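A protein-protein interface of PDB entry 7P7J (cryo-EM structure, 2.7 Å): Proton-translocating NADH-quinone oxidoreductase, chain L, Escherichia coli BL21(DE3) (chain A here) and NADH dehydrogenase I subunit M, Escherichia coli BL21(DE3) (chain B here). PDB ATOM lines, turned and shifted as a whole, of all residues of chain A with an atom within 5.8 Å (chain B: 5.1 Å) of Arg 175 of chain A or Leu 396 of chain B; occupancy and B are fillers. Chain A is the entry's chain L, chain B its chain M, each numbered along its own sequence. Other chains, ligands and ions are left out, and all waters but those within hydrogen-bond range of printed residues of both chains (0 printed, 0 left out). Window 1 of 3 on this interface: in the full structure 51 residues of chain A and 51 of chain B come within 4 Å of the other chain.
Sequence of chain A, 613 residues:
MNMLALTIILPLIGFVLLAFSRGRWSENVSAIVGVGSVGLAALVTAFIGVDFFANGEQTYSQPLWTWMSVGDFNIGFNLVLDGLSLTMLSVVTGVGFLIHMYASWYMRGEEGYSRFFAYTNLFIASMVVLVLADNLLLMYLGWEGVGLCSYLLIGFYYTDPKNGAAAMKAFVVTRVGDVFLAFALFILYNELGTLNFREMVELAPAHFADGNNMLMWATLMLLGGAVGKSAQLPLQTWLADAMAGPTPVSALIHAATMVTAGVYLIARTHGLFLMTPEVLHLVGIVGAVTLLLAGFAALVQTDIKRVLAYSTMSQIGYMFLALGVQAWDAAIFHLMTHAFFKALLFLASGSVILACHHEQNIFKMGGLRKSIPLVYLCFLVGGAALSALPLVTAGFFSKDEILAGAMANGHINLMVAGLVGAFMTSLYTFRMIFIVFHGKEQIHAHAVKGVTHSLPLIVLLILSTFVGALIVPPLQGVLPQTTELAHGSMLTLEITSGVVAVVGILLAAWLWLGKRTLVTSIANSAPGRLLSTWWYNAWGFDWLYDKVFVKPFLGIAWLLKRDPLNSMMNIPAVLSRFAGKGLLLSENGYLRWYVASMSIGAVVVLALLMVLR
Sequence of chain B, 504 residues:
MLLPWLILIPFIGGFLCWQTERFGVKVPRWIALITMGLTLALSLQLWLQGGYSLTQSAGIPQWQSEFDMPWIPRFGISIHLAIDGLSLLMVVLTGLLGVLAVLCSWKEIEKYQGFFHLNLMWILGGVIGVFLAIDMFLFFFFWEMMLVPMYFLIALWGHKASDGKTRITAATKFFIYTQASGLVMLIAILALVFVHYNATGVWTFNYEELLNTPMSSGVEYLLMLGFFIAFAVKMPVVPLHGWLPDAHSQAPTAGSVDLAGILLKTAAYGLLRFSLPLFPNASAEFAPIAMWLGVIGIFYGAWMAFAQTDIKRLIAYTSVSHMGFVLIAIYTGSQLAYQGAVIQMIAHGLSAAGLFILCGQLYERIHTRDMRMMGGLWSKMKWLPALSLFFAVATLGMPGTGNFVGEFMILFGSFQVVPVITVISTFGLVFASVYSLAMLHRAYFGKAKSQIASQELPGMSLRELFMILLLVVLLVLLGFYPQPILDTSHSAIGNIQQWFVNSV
Of the 13 printed residues of chain A, 5 touch a printed residue of chain B. Hydrophobic or aromatic side chains of chain A that line the printed part of chain B: Phe 171, Val 176 and Val 179. Among the printed residues, no Asp or Glu carboxylate lies within 4 Å of a Lys or Arg side-chain nitrogen of the other chain.
The backbone carbonyl oxygen (O) of Leu 396 of chain B is in hydrogen-bond range of the guanidinium group (NH2) of Arg 175 of chain A, at 2.8 Å. The side-chain sulfur (SD) of Met 398 of chain B lies close to the backbone carbonyl oxygen (O) of Glu 144 of chain A.
Tyr 140 of chain A touches none of the printed residues of chain B. Of the printed residues of chain B, Glu 144 of chain A touches Met 398 (3.2 Å). Printed residues of chain B within 4 Å of Phe 171 of chain A: Leu 396 (3.9 Å), Met 398 (3.97 Å), Ser 433 (3.7 Å) and Leu 437 (3.6 Å). Ala 392 of chain B touches none of the printed residues of chain A. Leu 396 of chain B touches just these residues of chain A: Phe 171 and Arg 175. Of the printed residues of chain A, Gly 397 of chain B touches Arg 175 (3.6 Å). Printed residues of chain A within 4 Å of Val 430 of chain B: Arg 175 (3.8 Å), Val 176 (3.9 Å) and Val 179 (3.6 Å). The nearest residue of chain B that does not touch Arg 175 of chain A is Met 398 of chain B (4.4 Å). The nearest residue of chain A that does not touch Leu 396 of chain B is Glu 144 of chain A (5.6 Å). The nearest printed residue of chain B that does not touch Glu 144 of chain A is Gly 397 of chain B (5.4 Å).
The backbone carbonyl oxygen (O) of Val 393 of chain B lies close to the backbone NH (N) of Met 398 of chain B. The side-chain hydroxyl of Ser 433 of chain B lies within hydrogen-bond range of the backbone carbonyl oxygen of Val 430 of chain B, at 2.7 Å. The side-chain carboxylate (OE2) of Glu 144 of chain A sits at hydrogen-bond distance from the side-chain hydroxyl (OH) of Tyr 140 of chain A (3.2 Å). The guanidinium group of Arg 175 of chain A lies within salt-bridge range of the side-chain carboxylate of Glu 144 of chain A, 2.4 Å away. The side-chain hydroxyl (OG1) of Thr 174 of chain A lies within hydrogen-bond range of the backbone carbonyl oxygen (O) of Phe 171 of chain A (3.0 Å).
CD1 of Leu 396 of chain B touches CZ of Phe 171 of chain A (3.9 Å). Phe 171 of chain A touches Met 398 of chain B. Ser 433 of chain B touches Phe 171 of chain A. CD2 of Phe 171 of chain A touches CD1 of Leu 437 of chain B, at 3.6 Å. Arg 175 of chain A touches Gly 397 of chain B (NH2 to O, 3.6 Å). CD2 of Leu 429 of chain B touches NH2 of Arg 175 of chain A (3.95 Å). Val 430 of chain B touches Arg 175 of chain A. Arg 175 of chain A touches Ser 433 of chain B (CG to OG, 3.6 Å). N of Val 176 of chain A touches CG2 of Val 430 of chain B, 3.9 Å away. Val 179 of chain A touches Val 430 of chain B.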
ATOM      1  N   TYR A 140      16.699   8.332 -35.012  1.00  0.00           N
ATOM      2  CA  TYR A 140      16.937   8.451 -33.579  1.00  0.00           C
ATOM      3  C   TYR A 140      18.361   8.054 -33.219  1.00  0.00           C
ATOM      4  O   TYR A 140      18.962   8.634 -32.307  1.00  0.00           O
ATOM      5  CB  TYR A 140      15.934   7.592 -32.813  1.00  0.00           C
ATOM      6  CG  TYR A 140      15.760   7.980 -31.368  1.00  0.00           C
ATOM      7  CD1 TYR A 140      16.557   7.423 -30.381  1.00  0.00           C
ATOM      8  CD2 TYR A 140      14.792   8.897 -30.986  1.00  0.00           C
ATOM      9  CE1 TYR A 140      16.399   7.770 -29.059  1.00  0.00           C
ATOM     10  CE2 TYR A 140      14.629   9.252 -29.666  1.00  0.00           C
ATOM     11  CZ  TYR A 140      15.437   8.686 -28.706  1.00  0.00           C
ATOM     12  OH  TYR A 140      15.280   9.032 -27.387  1.00  0.00           O
ATOM     13  N   GLU A 144      20.786  10.677 -31.362  1.00  0.00           N
ATOM     14  CA  GLU A 144      21.485  10.473 -30.105  1.00  0.00           C
ATOM     15  C   GLU A 144      22.992  10.470 -30.292  1.00  0.00           C
ATOM     16  O   GLU A 144      23.717  10.897 -29.391  1.00  0.00           O
ATOM     17  CB  GLU A 144      21.029   9.173 -29.462  1.00  0.00           C
ATOM     18  CG  GLU A 144      19.612   9.204 -28.955  1.00  0.00           C
ATOM     19  CD  GLU A 144      19.525   9.586 -27.496  1.00  0.00           C
ATOM     20  OE1 GLU A 144      20.536  10.064 -26.942  1.00  0.00           O
ATOM     21  OE2 GLU A 144      18.446   9.405 -26.896  1.00  0.00           O
ATOM     22  N   ALA A 170      24.241  20.364 -21.480  1.00  0.00           N
ATOM     23  CA  ALA A 170      23.811  20.218 -22.866  1.00  0.00           C
ATOM     24  C   ALA A 170      23.284  18.817 -23.136  1.00  0.00           C
ATOM     25  O   ALA A 170      22.222  18.655 -23.752  1.00  0.00           O
ATOM     26  CB  ALA A 170      24.966  20.545 -23.810  1.00  0.00           C
ATOM     27  N   PHE A 171      23.991  17.796 -22.646  1.00  0.00           N
ATOM     28  CA  PHE A 171      23.554  16.424 -22.873  1.00  0.00           C
ATOM     29  C   PHE A 171      22.256  16.119 -22.138  1.00  0.00           C
ATOM     30  O   PHE A 171      21.408  15.400 -22.666  1.00  0.00           O
ATOM     31  CB  PHE A 171      24.644  15.441 -22.461  1.00  0.00           C
ATOM     32  CG  PHE A 171      24.399  14.038 -22.935  1.00  0.00           C
ATOM     33  CD1 PHE A 171      24.669  13.680 -24.242  1.00  0.00           C
ATOM     34  CD2 PHE A 171      23.893  13.080 -22.075  1.00  0.00           C
ATOM     35  CE1 PHE A 171      24.444  12.393 -24.683  1.00  0.00           C
ATOM     36  CE2 PHE A 171      23.666  11.791 -22.508  1.00  0.00           C
ATOM     37  CZ  PHE A 171      23.941  11.447 -23.814  1.00  0.00           C
ATOM     38  N   VAL A 172      22.065  16.670 -20.937  1.00  0.00           N
ATOM     39  CA  VAL A 172      20.842  16.390 -20.187  1.00  0.00           C
ATOM     40  C   VAL A 172      19.635  17.060 -20.840  1.00  0.00           C
ATOM     41  O   VAL A 172      18.566  16.444 -20.976  1.00  0.00           O
ATOM     42  CB  VAL A 172      21.018  16.809 -18.715  1.00  0.00           C
ATOM     43  CG1 VAL A 172      19.680  16.918 -18.008  1.00  0.00           C
ATOM     44  CG2 VAL A 172      21.901  15.811 -17.996  1.00  0.00           C
ATOM     45  N   VAL A 173      19.784  18.317 -21.271  1.00  0.00           N
ATOM     46  CA  VAL A 173      18.678  19.008 -21.932  1.00  0.00           C
ATOM     47  C   VAL A 173      18.333  18.336 -23.258  1.00  0.00           C
ATOM     48  O   VAL A 173      17.153  18.077 -23.558  1.00  0.00           O
ATOM     49  CB  VAL A 173      19.021  20.496 -22.114  1.00  0.00           C
ATOM     50  CG1 VAL A 173      18.000  21.175 -22.998  1.00  0.00           C
ATOM     51  CG2 VAL A 173      19.085  21.186 -20.767  1.00  0.00           C
ATOM     52  N   THR A 174      19.349  18.000 -24.057  1.00  0.00           N
ATOM     53  CA  THR A 174      19.077  17.282 -25.291  1.00  0.00           C
ATOM     54  C   THR A 174      18.564  15.871 -25.040  1.00  0.00           C
ATOM     55  O   THR A 174      17.838  15.346 -25.876  1.00  0.00           O
ATOM     56  CB  THR A 174      20.324  17.242 -26.166  1.00  0.00           C
ATOM     57  OG1 THR A 174      21.420  16.714 -25.412  1.00  0.00           O
ATOM     58  CG2 THR A 174      20.664  18.642 -26.637  1.00  0.00           C
ATOM     59  N   ARG A 175      18.882  15.263 -23.896  1.00  0.00           N
ATOM     60  CA  ARG A 175      18.326  13.953 -23.581  1.00  0.00           C
ATOM     61  C   ARG A 175      16.851  14.044 -23.224  1.00  0.00           C
ATOM     62  O   ARG A 175      16.083  13.132 -23.542  1.00  0.00           O
ATOM     63  CB  ARG A 175      19.116  13.312 -22.443  1.00  0.00           C
ATOM     64  CG  ARG A 175      19.128  11.802 -22.476  1.00  0.00           C
ATOM     65  CD  ARG A 175      20.039  11.283 -23.570  1.00  0.00           C
ATOM     66  NE  ARG A 175      20.386   9.884 -23.353  1.00  0.00           N
ATOM     67  CZ  ARG A 175      19.668   8.860 -23.791  1.00  0.00           C
ATOM     68  NH1 ARG A 175      18.554   9.041 -24.480  1.00  0.00           N
ATOM     69  NH2 ARG A 175      20.077   7.623 -23.530  1.00  0.00           N
ATOM     70  N   VAL A 176      16.440  15.131 -22.568  1.00  0.00           N
ATOM     71  CA  VAL A 176      15.013  15.379 -22.360  1.00  0.00           C
ATOM     72  C   VAL A 176      14.307  15.550 -23.702  1.00  0.00           C
ATOM     73  O   VAL A 176      13.208  15.012 -23.927  1.00  0.00           O
ATOM     74  CB  VAL A 176      14.812  16.602 -21.446  1.00  0.00           C
ATOM     75  CG1 VAL A 176      13.348  16.976 -21.362  1.00  0.00           C
ATOM     76  CG2 VAL A 176      15.360  16.320 -20.062  1.00  0.00           C
ATOM     77  N   GLY A 177      14.941  16.285 -24.620  1.00  0.00           N
ATOM     78  CA  GLY A 177      14.399  16.393 -25.970  1.00  0.00           C
ATOM     79  C   GLY A 177      14.296  15.052 -26.679  1.00  0.00           C
ATOM     80  O   GLY A 177      13.289  14.754 -27.326  1.00  0.00           O
ATOM     81  N   ASP A 178      15.326  14.215 -26.546  1.00  0.00           N
ATOM     82  CA  ASP A 178      15.304  12.891 -27.159  1.00  0.00           C
ATOM     83  C   ASP A 178      14.259  11.990 -26.520  1.00  0.00           C
ATOM     84  O   ASP A 178      13.722  11.104 -27.185  1.00  0.00           O
ATOM     85  CB  ASP A 178      16.685  12.247 -27.071  1.00  0.00           C
ATOM     86  CG  ASP A 178      17.735  13.033 -27.822  1.00  0.00           C
ATOM     87  OD1 ASP A 178      17.395  14.118 -28.334  1.00  0.00           O
ATOM     88  OD2 ASP A 178      18.896  12.581 -27.891  1.00  0.00           O
ATOM     89  N   VAL A 179      13.951  12.206 -25.242  1.00  0.00           N
ATOM     90  CA  VAL A 179      12.887  11.449 -24.594  1.00  0.00           C
ATOM     91  C   VAL A 179      11.527  11.851 -25.154  1.00  0.00           C
ATOM     92  O   VAL A 179      10.655  11.000 -25.383  1.00  0.00           O
ATOM     93  CB  VAL A 179      12.984  11.636 -23.069  1.00  0.00           C
ATOM     94  CG1 VAL A 179      11.640  11.468 -22.382  1.00  0.00           C
ATOM     95  CG2 VAL A 179      13.991  10.661 -22.518  1.00  0.00           C
ATOM     96  N   PHE A 180      11.336  13.146 -25.413  1.00  0.00           N
ATOM     97  CA  PHE A 180      10.108  13.586 -26.082  1.00  0.00           C
ATOM     98  C   PHE A 180      10.005  13.003 -27.492  1.00  0.00           C
ATOM     99  O   PHE A 180       8.925  12.574 -27.929  1.00  0.00           O
ATOM    100  CB  PHE A 180      10.057  15.112 -26.129  1.00  0.00           C
ATOM    101  CG  PHE A 180       9.856  15.761 -24.788  1.00  0.00           C
ATOM    102  CD1 PHE A 180       9.388  15.038 -23.704  1.00  0.00           C
ATOM    103  CD2 PHE A 180      10.128  17.105 -24.617  1.00  0.00           C
ATOM    104  CE1 PHE A 180       9.198  15.639 -22.482  1.00  0.00           C
ATOM    105  CE2 PHE A 180       9.942  17.712 -23.394  1.00  0.00           C
ATOM    106  CZ  PHE A 180       9.476  16.976 -22.326  1.00  0.00           C
ATOM    107  N   ALA B 392      30.128   3.472 -20.147  1.00  0.00           N
ATOM    108  CA  ALA B 392      29.148   4.370 -19.549  1.00  0.00           C
ATOM    109  C   ALA B 392      28.167   4.898 -20.585  1.00  0.00           C
ATOM    110  O   ALA B 392      26.987   5.096 -20.276  1.00  0.00           O
ATOM    111  CB  ALA B 392      29.852   5.529 -18.857  1.00  0.00           C
ATOM    112  N   VAL B 393      28.642   5.154 -21.805  1.00  0.00           N
ATOM    113  CA  VAL B 393      27.757   5.504 -22.910  1.00  0.00           C
ATOM    114  C   VAL B 393      26.818   4.346 -23.234  1.00  0.00           C
ATOM    115  O   VAL B 393      25.637   4.549 -23.537  1.00  0.00           O
ATOM    116  CB  VAL B 393      28.609   5.939 -24.117  1.00  0.00           C
ATOM    117  CG1 VAL B 393      27.818   5.949 -25.385  1.00  0.00           C
ATOM    118  CG2 VAL B 393      29.157   7.330 -23.875  1.00  0.00           C
ATOM    119  N   ALA B 394      27.323   3.116 -23.152  1.00  0.00           N
ATOM    120  CA  ALA B 394      26.486   1.943 -23.378  1.00  0.00           C
ATOM    121  C   ALA B 394      25.407   1.809 -22.311  1.00  0.00           C
ATOM    122  O   ALA B 394      24.248   1.526 -22.630  1.00  0.00           O
ATOM    123  CB  ALA B 394      27.352   0.685 -23.421  1.00  0.00           C
ATOM    124  N   THR B 395      25.761   2.022 -21.040  1.00  0.00           N
ATOM    125  CA  THR B 395      24.797   1.798 -19.967  1.00  0.00           C
ATOM    126  C   THR B 395      23.719   2.871 -19.897  1.00  0.00           C
ATOM    127  O   THR B 395      22.678   2.638 -19.275  1.00  0.00           O
ATOM    128  CB  THR B 395      25.501   1.698 -18.616  1.00  0.00           C
ATOM    129  OG1 THR B 395      26.405   2.798 -18.460  1.00  0.00           O
ATOM    130  CG2 THR B 395      26.265   0.390 -18.517  1.00  0.00           C
ATOM    131  N   LEU B 396      23.927   4.033 -20.513  1.00  0.00           N
ATOM    132  CA  LEU B 396      22.862   5.027 -20.542  1.00  0.00           C
ATOM    133  C   LEU B 396      21.892   4.811 -21.694  1.00  0.00           C
ATOM    134  O   LEU B 396      20.965   5.609 -21.858  1.00  0.00           O
ATOM    135  CB  LEU B 396      23.437   6.449 -20.594  1.00  0.00           C
ATOM    136  CG  LEU B 396      24.276   6.965 -21.763  1.00  0.00           C
ATOM    137  CD1 LEU B 396      23.433   7.710 -22.780  1.00  0.00           C
ATOM    138  CD2 LEU B 396      25.363   7.876 -21.235  1.00  0.00           C
ATOM    139  N   GLY B 397      22.081   3.765 -22.494  1.00  0.00           N
ATOM    140  CA  GLY B 397      21.133   3.435 -23.535  1.00  0.00           C
ATOM    141  C   GLY B 397      21.373   4.188 -24.823  1.00  0.00           C
ATOM    142  O   GLY B 397      20.424   4.584 -25.505  1.00  0.00           O
ATOM    143  N   MET B 398      22.630   4.409 -25.155  1.00  0.00           N
ATOM    144  CA  MET B 398      22.957   5.102 -26.391  1.00  0.00           C
ATOM    145  C   MET B 398      22.823   4.151 -27.573  1.00  0.00           C
ATOM    146  O   MET B 398      23.247   2.996 -27.479  1.00  0.00           O
ATOM    147  CB  MET B 398      24.374   5.661 -26.334  1.00  0.00           C
ATOM    148  CG  MET B 398      24.877   6.343 -27.610  1.00  0.00           C
ATOM    149  SD  MET B 398      24.237   7.971 -28.085  1.00  0.00           S
ATOM    150  CE  MET B 398      23.511   8.625 -26.580  1.00  0.00           C
ATOM    151  N   GLU B 407      16.245  -1.868 -24.513  1.00  0.00           N
ATOM    152  CA  GLU B 407      15.355  -1.015 -23.733  1.00  0.00           C
ATOM    153  C   GLU B 407      14.334  -0.308 -24.613  1.00  0.00           C
ATOM    154  O   GLU B 407      13.227  -0.014 -24.155  1.00  0.00           O
ATOM    155  CB  GLU B 407      16.165  -0.004 -22.928  1.00  0.00           C
ATOM    156  CG  GLU B 407      16.833   1.052 -23.765  1.00  0.00           C
ATOM    157  CD  GLU B 407      17.124   2.297 -22.995  1.00  0.00           C
ATOM    158  OE1 GLU B 407      16.747   2.350 -21.807  1.00  0.00           O
ATOM    159  OE2 GLU B 407      17.753   3.205 -23.577  1.00  0.00           O
ATOM    160  N   LEU B 429      15.218   6.971 -18.163  1.00  0.00           N
ATOM    161  CA  LEU B 429      16.329   6.995 -19.118  1.00  0.00           C
ATOM    162  C   LEU B 429      17.107   8.306 -19.042  1.00  0.00           C
ATOM    163  O   LEU B 429      18.347   8.315 -19.140  1.00  0.00           O
ATOM    164  CB  LEU B 429      15.814   6.780 -20.537  1.00  0.00           C
ATOM    165  CG  LEU B 429      16.232   5.519 -21.262  1.00  0.00           C
ATOM    166  CD1 LEU B 429      15.716   5.583 -22.683  1.00  0.00           C
ATOM    167  CD2 LEU B 429      17.741   5.424 -21.223  1.00  0.00           C
ATOM    168  N   VAL B 430      16.387   9.427 -18.907  1.00  0.00           N
ATOM    169  CA  VAL B 430      17.050  10.713 -18.642  1.00  0.00           C
ATOM    170  C   VAL B 430      17.917  10.621 -17.388  1.00  0.00           C
ATOM    171  O   VAL B 430      19.080  11.056 -17.372  1.00  0.00           O
ATOM    172  CB  VAL B 430      16.017  11.852 -18.528  1.00  0.00           C
ATOM    173  CG1 VAL B 430      16.563  13.013 -17.710  1.00  0.00           C
ATOM    174  CG2 VAL B 430      15.674  12.373 -19.882  1.00  0.00           C
ATOM    175  N   ALA B 432      19.245   7.968 -16.139  1.00  0.00           N
ATOM    176  CA  ALA B 432      20.375   7.094 -16.438  1.00  0.00           C
ATOM    177  C   ALA B 432      21.507   7.858 -17.102  1.00  0.00           C
ATOM    178  O   ALA B 432      22.683   7.687 -16.741  1.00  0.00           O
ATOM    179  CB  ALA B 432      19.923   5.936 -17.323  1.00  0.00           C
ATOM    180  N   SER B 433      21.168   8.709 -18.074  1.00  0.00           N
ATOM    181  CA  SER B 433      22.182   9.564 -18.688  1.00  0.00           C
ATOM    182  C   SER B 433      22.809  10.495 -17.657  1.00  0.00           C
ATOM    183  O   SER B 433      24.024  10.742 -17.688  1.00  0.00           O
ATOM    184  CB  SER B 433      21.576  10.367 -19.836  1.00  0.00           C
ATOM    185  OG  SER B 433      20.854  11.480 -19.348  1.00  0.00           O
ATOM    186  N   SER B 436      25.299   8.409 -15.455  1.00  0.00           N
ATOM    187  CA  SER B 436      26.458   7.994 -16.242  1.00  0.00           C
ATOM    188  C   SER B 436      27.410   9.160 -16.478  1.00  0.00           C
ATOM    189  O   SER B 436      28.630   9.027 -16.296  1.00  0.00           O
ATOM    190  CB  SER B 436      26.005   7.395 -17.570  1.00  0.00           C
ATOM    191  OG  SER B 436      25.228   6.231 -17.359  1.00  0.00           O
ATOM    192  N   LEU B 437      26.863  10.326 -16.840  1.00  0.00           N
ATOM    193  CA  LEU B 437      27.705  11.503 -17.012  1.00  0.00           C
ATOM    194  C   LEU B 437      28.313  11.962 -15.696  1.00  0.00           C
ATOM    195  O   LEU B 437      29.447  12.451 -15.685  1.00  0.00           O
ATOM    196  CB  LEU B 437      26.904  12.638 -17.642  1.00  0.00           C
ATOM    197  CG  LEU B 437      26.529  12.519 -19.118  1.00  0.00           C
ATOM    198  CD1 LEU B 437      26.448  13.906 -19.694  1.00  0.00           C
ATOM    199  CD2 LEU B 437      27.517  11.668 -19.902  1.00  0.00           C
